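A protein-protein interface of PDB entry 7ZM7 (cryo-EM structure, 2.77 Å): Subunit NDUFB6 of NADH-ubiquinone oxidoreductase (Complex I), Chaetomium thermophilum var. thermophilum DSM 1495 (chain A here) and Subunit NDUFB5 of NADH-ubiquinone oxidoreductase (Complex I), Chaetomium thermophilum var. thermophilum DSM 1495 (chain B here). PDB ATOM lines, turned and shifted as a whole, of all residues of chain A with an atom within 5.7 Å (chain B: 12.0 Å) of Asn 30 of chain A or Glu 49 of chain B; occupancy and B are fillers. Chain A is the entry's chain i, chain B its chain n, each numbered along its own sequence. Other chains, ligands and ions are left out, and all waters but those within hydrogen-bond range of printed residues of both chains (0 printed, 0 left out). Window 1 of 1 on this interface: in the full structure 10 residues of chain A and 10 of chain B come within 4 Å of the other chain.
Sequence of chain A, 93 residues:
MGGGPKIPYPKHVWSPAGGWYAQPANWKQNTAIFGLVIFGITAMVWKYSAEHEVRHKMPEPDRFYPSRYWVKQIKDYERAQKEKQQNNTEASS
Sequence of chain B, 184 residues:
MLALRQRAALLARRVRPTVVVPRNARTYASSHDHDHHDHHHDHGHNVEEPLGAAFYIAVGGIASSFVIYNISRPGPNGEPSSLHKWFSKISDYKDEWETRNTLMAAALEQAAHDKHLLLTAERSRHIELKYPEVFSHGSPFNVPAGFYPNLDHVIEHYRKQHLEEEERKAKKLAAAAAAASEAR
CE1 of His 45 of chain B touches C of Pro 24 of chain A (3.98 Å).
O of Val 47 of chain B touches CA of Pro 24 of chain A (3.9 Å).
Glu 49 of chain B touches Pro 24 of chain A (CG to CB, 3.9 Å).
CE1 of His 45 of chain B touches N of Ala 25 of chain A, 3.8 Å away.
Ala 25 of chain A touches Asn 46 of chain B (CB to CA, 3.7 Å).
Ala 25 of chain A touches Glu 48 of chain B (CB to CG, 3.8 Å).
Glu 48 of chain B touches Asn 26 of chain A (CA to OD1, 2.9 Å).
Ile 33 of chain A touches Leu 51 of chain B.
Phe 55 of chain B touches Ile 33 of chain A.
Phe 34 of chain A touches Phe 55 of chain B (CE1 to CD1, 3.7 Å).
The side-chain amide nitrogen of Asn 26 of chain A is in hydrogen-bond range of the side-chain amide oxygen of Asn 30 of chain A (2.6 Å).
A ring nitrogen (ND1) of His 45 of chain B lies within hydrogen-bond range of the backbone NH (N) of Val 47 of chain B (3.3 Å).
The backbone carbonyl oxygen of Asn 26 of chain A sits close to the side-chain amide oxygen of Gln 29 of chain A, 2.9 Å away.
Along chain A the printed residues that touch a printed residue of chain B span positions 24 to 34.
Among the printed residues, 15 pairs touch across the chains.
Among the printed residues, no Asp or Glu carboxylate lies within 4 Å of a Lys or Arg side-chain nitrogen of the other chain.
Asn 30 of chain A touches just these residues of chain B: Glu 49 (3.1 Å) and Leu 51 (3.1 Å).
Of chain A, only Pro 24 (3.9 Å), Asn 26 (2.5 Å) and Asn 30 (3.1 Å) come within 4 Å of Glu 49 of chain B.
Pro 24 of chain A touches three residues of chain B.
Of chain B, only His 45 (3.8 Å), Asn 46 (3.7 Å), Val 47 (3.2 Å) and Glu 48 (3.8 Å) come within 4 Å of Ala 25 of chain A.
Of chain B, only Glu 48 (2.9 Å) and Glu 49 (2.5 Å) come within 4 Å of Asn 26 of chain A.
No residue of chain B comes within 4 Å of Thr 31 of chain A.
Of chain B, only Leu 51 and Phe 55 come within 4 Å of Ile 33 of chain A.
Of the printed residues of chain A, Phe 55 of chain B touches Ile 33 and Phe 34.
Of the printed residues of chain A, His 45 of chain B touches Pro 24 and Ala 25.
Printed residues of chain A within 4 Å of Glu 48 of chain B: Ala 25 (3.8 Å) and Asn 26 (2.9 Å).
The nearest residue of chain B that does not touch Asn 30 of chain A is Pro 50 of chain B (4.9 Å).
The nearest printed residue of chain A that does not touch Val 47 of chain B is Asn 26 of chain A (4.5 Å).
The side-chain amide oxygen (OD1) of Asn 30 of chain A lies close to the backbone carbonyl oxygen (O) of Glu 49 of chain B (3.1 Å).
N of Glu 49 of chain B is in hydrogen-bond range of OD1 of Asn 26 of chain A (2.5 Å).
The backbone carbonyl oxygen of Val 47 of chain B lies within hydrogen-bond range of the backbone NH of Ala 25 of chain A (3.2 Å).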
ATOM      1  N   PRO A  24       2.852  15.819 -20.567  1.00  0.00           N
ATOM      2  CA  PRO A  24       3.984  16.706 -20.364  1.00  0.00           C
ATOM      3  C   PRO A  24       3.803  18.008 -21.154  1.00  0.00           C
ATOM      4  O   PRO A  24       2.917  18.071 -21.963  1.00  0.00           O
ATOM      5  CB  PRO A  24       5.175  15.895 -20.896  1.00  0.00           C
ATOM      6  CG  PRO A  24       4.568  14.943 -21.898  1.00  0.00           C
ATOM      7  CD  PRO A  24       3.172  14.656 -21.388  1.00  0.00           C
ATOM      8  N   ALA A  25       4.618  19.018 -20.867  1.00  0.00           N
ATOM      9  CA  ALA A  25       4.594  20.275 -21.634  1.00  0.00           C
ATOM     10  C   ALA A  25       5.205  20.003 -22.998  1.00  0.00           C
ATOM     11  O   ALA A  25       4.673  20.515 -23.997  1.00  0.00           O
ATOM     12  CB  ALA A  25       5.370  21.319 -20.893  1.00  0.00           C
ATOM     13  N   ASN A  26       6.277  19.210 -23.034  1.00  0.00           N
ATOM     14  CA  ASN A  26       7.000  19.042 -24.281  1.00  0.00           C
ATOM     15  C   ASN A  26       6.390  17.970 -25.161  1.00  0.00           C
ATOM     16  O   ASN A  26       7.061  17.464 -26.067  1.00  0.00           O
ATOM     17  CB  ASN A  26       8.469  18.730 -24.001  1.00  0.00           C
ATOM     18  CG  ASN A  26       8.658  17.472 -23.186  1.00  0.00           C
ATOM     19  OD1 ASN A  26       8.230  17.395 -22.051  1.00  0.00           O
ATOM     20  ND2 ASN A  26       9.336  16.492 -23.756  1.00  0.00           N
ATOM     21  N   TRP A  27       5.118  17.649 -24.939  1.00  0.00           N
ATOM     22  CA  TRP A  27       4.509  16.477 -25.550  1.00  0.00           C
ATOM     23  C   TRP A  27       4.447  16.570 -27.064  1.00  0.00           C
ATOM     24  O   TRP A  27       4.501  15.542 -27.743  1.00  0.00           O
ATOM     25  CB  TRP A  27       3.120  16.276 -24.967  1.00  0.00           C
ATOM     26  CG  TRP A  27       2.141  17.316 -25.334  1.00  0.00           C
ATOM     27  CD1 TRP A  27       1.854  18.435 -24.637  1.00  0.00           C
ATOM     28  CD2 TRP A  27       1.299  17.333 -26.482  1.00  0.00           C
ATOM     29  NE1 TRP A  27       0.886  19.154 -25.271  1.00  0.00           N
ATOM     30  CE2 TRP A  27       0.533  18.500 -26.416  1.00  0.00           C
ATOM     31  CE3 TRP A  27       1.116  16.471 -27.561  1.00  0.00           C
ATOM     32  CZ2 TRP A  27      -0.405  18.818 -27.369  1.00  0.00           C
ATOM     33  CZ3 TRP A  27       0.211  16.799 -28.505  1.00  0.00           C
ATOM     34  CH2 TRP A  27      -0.545  17.961 -28.410  1.00  0.00           C
ATOM     35  N   LYS A  28       4.311  17.773 -27.616  1.00  0.00           N
ATOM     36  CA  LYS A  28       4.286  17.901 -29.064  1.00  0.00           C
ATOM     37  C   LYS A  28       5.626  17.519 -29.667  1.00  0.00           C
ATOM     38  O   LYS A  28       5.682  16.941 -30.757  1.00  0.00           O
ATOM     39  CB  LYS A  28       3.897  19.315 -29.460  1.00  0.00           C
ATOM     40  CG  LYS A  28       2.504  19.698 -29.050  1.00  0.00           C
ATOM     41  CD  LYS A  28       2.152  21.076 -29.559  1.00  0.00           C
ATOM     42  CE  LYS A  28       0.759  21.493 -29.131  1.00  0.00           C
ATOM     43  NZ  LYS A  28       0.714  21.852 -27.688  1.00  0.00           N
ATOM     44  N   GLN A  29       6.716  17.833 -28.978  1.00  0.00           N
ATOM     45  CA  GLN A  29       8.031  17.444 -29.468  1.00  0.00           C
ATOM     46  C   GLN A  29       8.249  15.948 -29.316  1.00  0.00           C
ATOM     47  O   GLN A  29       8.739  15.287 -30.234  1.00  0.00           O
ATOM     48  CB  GLN A  29       9.107  18.245 -28.746  1.00  0.00           C
ATOM     49  CG  GLN A  29       9.064  19.727 -29.083  1.00  0.00           C
ATOM     50  CD  GLN A  29       8.024  20.488 -28.289  1.00  0.00           C
ATOM     51  OE1 GLN A  29       7.537  20.015 -27.266  1.00  0.00           O
ATOM     52  NE2 GLN A  29       7.664  21.670 -28.771  1.00  0.00           N
ATOM     53  N   ASN A  30       7.863  15.390 -28.173  1.00  0.00           N
ATOM     54  CA  ASN A  30       7.925  13.946 -28.007  1.00  0.00           C
ATOM     55  C   ASN A  30       7.023  13.233 -29.014  1.00  0.00           C
ATOM     56  O   ASN A  30       7.428  12.239 -29.622  1.00  0.00           O
ATOM     57  CB  ASN A  30       7.550  13.585 -26.575  1.00  0.00           C
ATOM     58  CG  ASN A  30       8.673  13.858 -25.596  1.00  0.00           C
ATOM     59  OD1 ASN A  30       8.443  14.189 -24.435  1.00  0.00           O
ATOM     60  ND2 ASN A  30       9.902  13.725 -26.065  1.00  0.00           N
ATOM     61  N   THR A  31       5.805  13.737 -29.215  1.00  0.00           N
ATOM     62  CA  THR A  31       4.898  13.119 -30.179  1.00  0.00           C
ATOM     63  C   THR A  31       5.473  13.156 -31.583  1.00  0.00           C
ATOM     64  O   THR A  31       5.430  12.154 -32.306  1.00  0.00           O
ATOM     65  CB  THR A  31       3.544  13.814 -30.159  1.00  0.00           C
ATOM     66  OG1 THR A  31       3.013  13.794 -28.827  1.00  0.00           O
ATOM     67  CG2 THR A  31       2.580  13.143 -31.118  1.00  0.00           C
ATOM     68  N   ALA A  32       6.029  14.296 -31.985  1.00  0.00           N
ATOM     69  CA  ALA A  32       6.614  14.397 -33.314  1.00  0.00           C
ATOM     70  C   ALA A  32       7.735  13.391 -33.500  1.00  0.00           C
ATOM     71  O   ALA A  32       7.800  12.715 -34.531  1.00  0.00           O
ATOM     72  CB  ALA A  32       7.128  15.812 -33.548  1.00  0.00           C
ATOM     73  N   ILE A  33       8.620  13.266 -32.512  1.00  0.00           N
ATOM     74  CA  ILE A  33       9.731  12.324 -32.618  1.00  0.00           C
ATOM     75  C   ILE A  33       9.217  10.902 -32.774  1.00  0.00           C
ATOM     76  O   ILE A  33       9.715  10.131 -33.599  1.00  0.00           O
ATOM     77  CB  ILE A  33      10.659  12.454 -31.397  1.00  0.00           C
ATOM     78  CG1 ILE A  33      11.213  13.872 -31.296  1.00  0.00           C
ATOM     79  CG2 ILE A  33      11.779  11.446 -31.462  1.00  0.00           C
ATOM     80  CD1 ILE A  33      12.036  14.287 -32.480  1.00  0.00           C
ATOM     81  N   PHE A  34       8.203  10.533 -31.992  1.00  0.00           N
ATOM     82  CA  PHE A  34       7.642   9.195 -32.118  1.00  0.00           C
ATOM     83  C   PHE A  34       7.006   8.981 -33.475  1.00  0.00           C
ATOM     84  O   PHE A  34       6.971   7.851 -33.964  1.00  0.00           O
ATOM     85  CB  PHE A  34       6.625   8.941 -31.014  1.00  0.00           C
ATOM     86  CG  PHE A  34       7.222   8.344 -29.799  1.00  0.00           C
ATOM     87  CD1 PHE A  34       7.873   7.136 -29.867  1.00  0.00           C
ATOM     88  CD2 PHE A  34       7.157   8.995 -28.590  1.00  0.00           C
ATOM     89  CE1 PHE A  34       8.442   6.580 -28.745  1.00  0.00           C
ATOM     90  CE2 PHE A  34       7.724   8.449 -27.464  1.00  0.00           C
ATOM     91  CZ  PHE A  34       8.372   7.245 -27.542  1.00  0.00           C
ATOM     92  N   GLY A  35       6.493  10.040 -34.091  1.00  0.00           N
ATOM     93  CA  GLY A  35       5.900   9.894 -35.406  1.00  0.00           C
ATOM     94  C   GLY A  35       6.913   9.484 -36.453  1.00  0.00           C
ATOM     95  O   GLY A  35       6.632   8.645 -37.307  1.00  0.00           O
ATOM     96  N   HIS B  45       1.242  23.775 -16.946  1.00  0.00           N
ATOM     97  CA  HIS B  45       2.545  23.560 -16.272  1.00  0.00           C
ATOM     98  C   HIS B  45       3.654  23.519 -17.317  1.00  0.00           C
ATOM     99  O   HIS B  45       3.332  23.666 -18.508  1.00  0.00           O
ATOM    100  CB  HIS B  45       2.518  22.277 -15.446  1.00  0.00           C
ATOM    101  CG  HIS B  45       2.202  21.066 -16.257  1.00  0.00           C
ATOM    102  ND1 HIS B  45       3.158  20.405 -16.997  1.00  0.00           N
ATOM    103  CD2 HIS B  45       1.044  20.402 -16.453  1.00  0.00           C
ATOM    104  CE1 HIS B  45       2.601  19.395 -17.624  1.00  0.00           C
ATOM    105  NE2 HIS B  45       1.308  19.368 -17.302  1.00  0.00           N
ATOM    106  N   ASN B  46       4.900  23.332 -16.880  1.00  0.00           N
ATOM    107  CA  ASN B  46       6.058  23.224 -17.798  1.00  0.00           C
ATOM    108  C   ASN B  46       6.997  22.136 -17.270  1.00  0.00           C
ATOM    109  O   ASN B  46       8.219  22.361 -17.312  1.00  0.00           O
ATOM    110  CB  ASN B  46       6.829  24.539 -17.867  1.00  0.00           C
ATOM    111  CG  ASN B  46       5.970  25.713 -18.282  1.00  0.00           C
ATOM    112  OD1 ASN B  46       5.555  25.809 -19.435  1.00  0.00           O
ATOM    113  ND2 ASN B  46       5.699  26.613 -17.352  1.00  0.00           N
ATOM    114  N   VAL B  47       6.405  21.094 -16.717  1.00  0.00           N
ATOM    115  CA  VAL B  47       7.217  19.936 -16.290  1.00  0.00           C
ATOM    116  C   VAL B  47       7.368  19.179 -17.586  1.00  0.00           C
ATOM    117  O   VAL B  47       6.349  18.852 -18.201  1.00  0.00           O
ATOM    118  CB  VAL B  47       6.497  19.080 -15.241  1.00  0.00           C
ATOM    119  CG1 VAL B  47       7.329  17.874 -14.835  1.00  0.00           C
ATOM    120  CG2 VAL B  47       6.125  19.907 -14.022  1.00  0.00           C
ATOM    121  N   GLU B  48       8.601  19.009 -18.027  1.00  0.00           N
ATOM    122  CA  GLU B  48       8.801  18.387 -19.334  1.00  0.00           C
ATOM    123  C   GLU B  48       9.248  16.956 -19.097  1.00  0.00           C
ATOM    124  O   GLU B  48       9.503  16.601 -17.948  1.00  0.00           O
ATOM    125  CB  GLU B  48       9.713  19.291 -20.140  1.00  0.00           C
ATOM    126  CG  GLU B  48       9.044  20.584 -20.560  1.00  0.00           C
ATOM    127  CD  GLU B  48       9.724  21.315 -21.704  1.00  0.00           C
ATOM    128  OE1 GLU B  48      10.896  20.999 -21.995  1.00  0.00           O
ATOM    129  OE2 GLU B  48       9.075  22.188 -22.310  1.00  0.00           O
ATOM    130  N   GLU B  49       9.286  16.154 -20.152  1.00  0.00           N
ATOM    131  CA  GLU B  49       9.642  14.720 -20.032  1.00  0.00           C
ATOM    132  C   GLU B  49      10.765  14.420 -21.010  1.00  0.00           C
ATOM    133  O   GLU B  49      10.570  14.638 -22.202  1.00  0.00           O
ATOM    134  CB  GLU B  49       8.446  13.845 -20.417  1.00  0.00           C
ATOM    135  CG  GLU B  49       7.616  13.396 -19.239  1.00  0.00           C
ATOM    136  CD  GLU B  49       8.286  12.354 -18.366  1.00  0.00           C
ATOM    137  OE1 GLU B  49       8.835  11.389 -18.922  1.00  0.00           O
ATOM    138  OE2 GLU B  49       8.265  12.521 -17.135  1.00  0.00           O
ATOM    139  N   PRO B  50      11.930  13.931 -20.569  1.00  0.00           N
ATOM    140  CA  PRO B  50      12.945  13.507 -21.521  1.00  0.00           C
ATOM    141  C   PRO B  50      12.459  12.203 -22.166  1.00  0.00           C
ATOM    142  O   PRO B  50      11.888  11.441 -21.470  1.00  0.00           O
ATOM    143  CB  PRO B  50      14.184  13.317 -20.636  1.00  0.00           C
ATOM    144  CG  PRO B  50      13.636  13.055 -19.246  1.00  0.00           C
ATOM    145  CD  PRO B  50      12.328  13.814 -19.170  1.00  0.00           C
ATOM    146  N   LEU B  51      12.773  11.964 -23.432  1.00  0.00           N
ATOM    147  CA  LEU B  51      12.329  10.739 -24.151  1.00  0.00           C
ATOM    148  C   LEU B  51      12.865   9.531 -23.382  1.00  0.00           C
ATOM    149  O   LEU B  51      12.223   8.475 -23.424  1.00  0.00           O
ATOM    150  CB  LEU B  51      12.800  10.754 -25.609  1.00  0.00           C
ATOM    151  CG  LEU B  51      11.853  11.383 -26.620  1.00  0.00           C
ATOM    152  CD1 LEU B  51      12.601  11.788 -27.876  1.00  0.00           C
ATOM    153  CD2 LEU B  51      10.714  10.438 -26.948  1.00  0.00           C
ATOM    154  N   GLY B  52      14.054   9.652 -22.806  1.00  0.00           N
ATOM    155  CA  GLY B  52      14.538   8.595 -21.906  1.00  0.00           C
ATOM    156  C   GLY B  52      15.478   7.589 -22.520  1.00  0.00           C
ATOM    157  O   GLY B  52      15.525   7.466 -23.743  1.00  0.00           O
ATOM    158  N   ALA B  53      16.194   6.879 -21.659  1.00  0.00           N
ATOM    159  CA  ALA B  53      17.067   5.817 -22.139  1.00  0.00           C
ATOM    160  C   ALA B  53      16.298   4.688 -22.803  1.00  0.00           C
ATOM    161  O   ALA B  53      16.756   4.146 -23.814  1.00  0.00           O
ATOM    162  CB  ALA B  53      17.887   5.259 -20.980  1.00  0.00           C
ATOM    163  N   ALA B  54      15.144   4.315 -22.250  1.00  0.00           N
ATOM    164  CA  ALA B  54      14.375   3.210 -22.805  1.00  0.00           C
ATOM    165  C   ALA B  54      14.002   3.471 -24.252  1.00  0.00           C
ATOM    166  O   ALA B  54      13.960   2.543 -25.067  1.00  0.00           O
ATOM    167  CB  ALA B  54      13.122   2.974 -21.968  1.00  0.00           C
ATOM    168  N   PHE B  55      13.726   4.730 -24.593  1.00  0.00           N
ATOM    169  CA  PHE B  55      13.448   5.073 -25.978  1.00  0.00           C
ATOM    170  C   PHE B  55      14.648   4.791 -26.868  1.00  0.00           C
ATOM    171  O   PHE B  55      14.503   4.258 -27.972  1.00  0.00           O
ATOM    172  CB  PHE B  55      13.051   6.536 -26.071  1.00  0.00           C
ATOM    173  CG  PHE B  55      13.073   7.075 -27.449  1.00  0.00           C
ATOM    174  CD1 PHE B  55      12.150   6.656 -28.380  1.00  0.00           C
ATOM    175  CD2 PHE B  55      14.006   8.016 -27.815  1.00  0.00           C
ATOM    176  CE1 PHE B  55      12.165   7.157 -29.659  1.00  0.00           C
ATOM    177  CE2 PHE B  55      14.028   8.520 -29.090  1.00  0.00           C
ATOM    178  CZ  PHE B  55      13.106   8.091 -30.014  1.00  0.00           C
ATOM    179  N   TYR B  56      15.847   5.130 -26.398  1.00  0.00           N
ATOM    180  CA  TYR B  56      17.030   4.982 -27.230  1.00  0.00           C
ATOM    181  C   TYR B  56      17.463   3.528 -27.330  1.00  0.00           C
ATOM    182  O   TYR B  56      17.946   3.091 -28.379  1.00  0.00           O
ATOM    183  CB  TYR B  56      18.158   5.847 -26.680  1.00  0.00           C
ATOM    184  CG  TYR B  56      17.942   7.322 -26.903  1.00  0.00           C
ATOM    185  CD1 TYR B  56      17.874   7.844 -28.183  1.00  0.00           C
ATOM    186  CD2 TYR B  56      17.796   8.190 -25.836  1.00  0.00           C
ATOM    187  CE1 TYR B  56      17.673   9.186 -28.393  1.00  0.00           C
ATOM    188  CE2 TYR B  56      17.595   9.533 -26.035  1.00  0.00           C
ATOM    189  CZ  TYR B  56      17.535  10.027 -27.314  1.00  0.00           C
ATOM    190  OH  TYR B  56      17.334  11.373 -27.519  1.00  0.00           O
ATOM    191  N   VAL B  59      15.042   1.998 -29.769  1.00  0.00           N
ATOM    192  CA  VAL B  59      15.339   2.430 -31.126  1.00  0.00           C
ATOM    193  C   VAL B  59      16.711   1.944 -31.545  1.00  0.00           C
ATOM    194  O   VAL B  59      16.886   1.403 -32.638  1.00  0.00           O
ATOM    195  CB  VAL B  59      15.218   3.960 -31.237  1.00  0.00           C
ATOM    196  CG1 VAL B  59      15.781   4.448 -32.562  1.00  0.00           C
ATOM    197  CG2 VAL B  59      13.770   4.382 -31.088  1.00  0.00           C
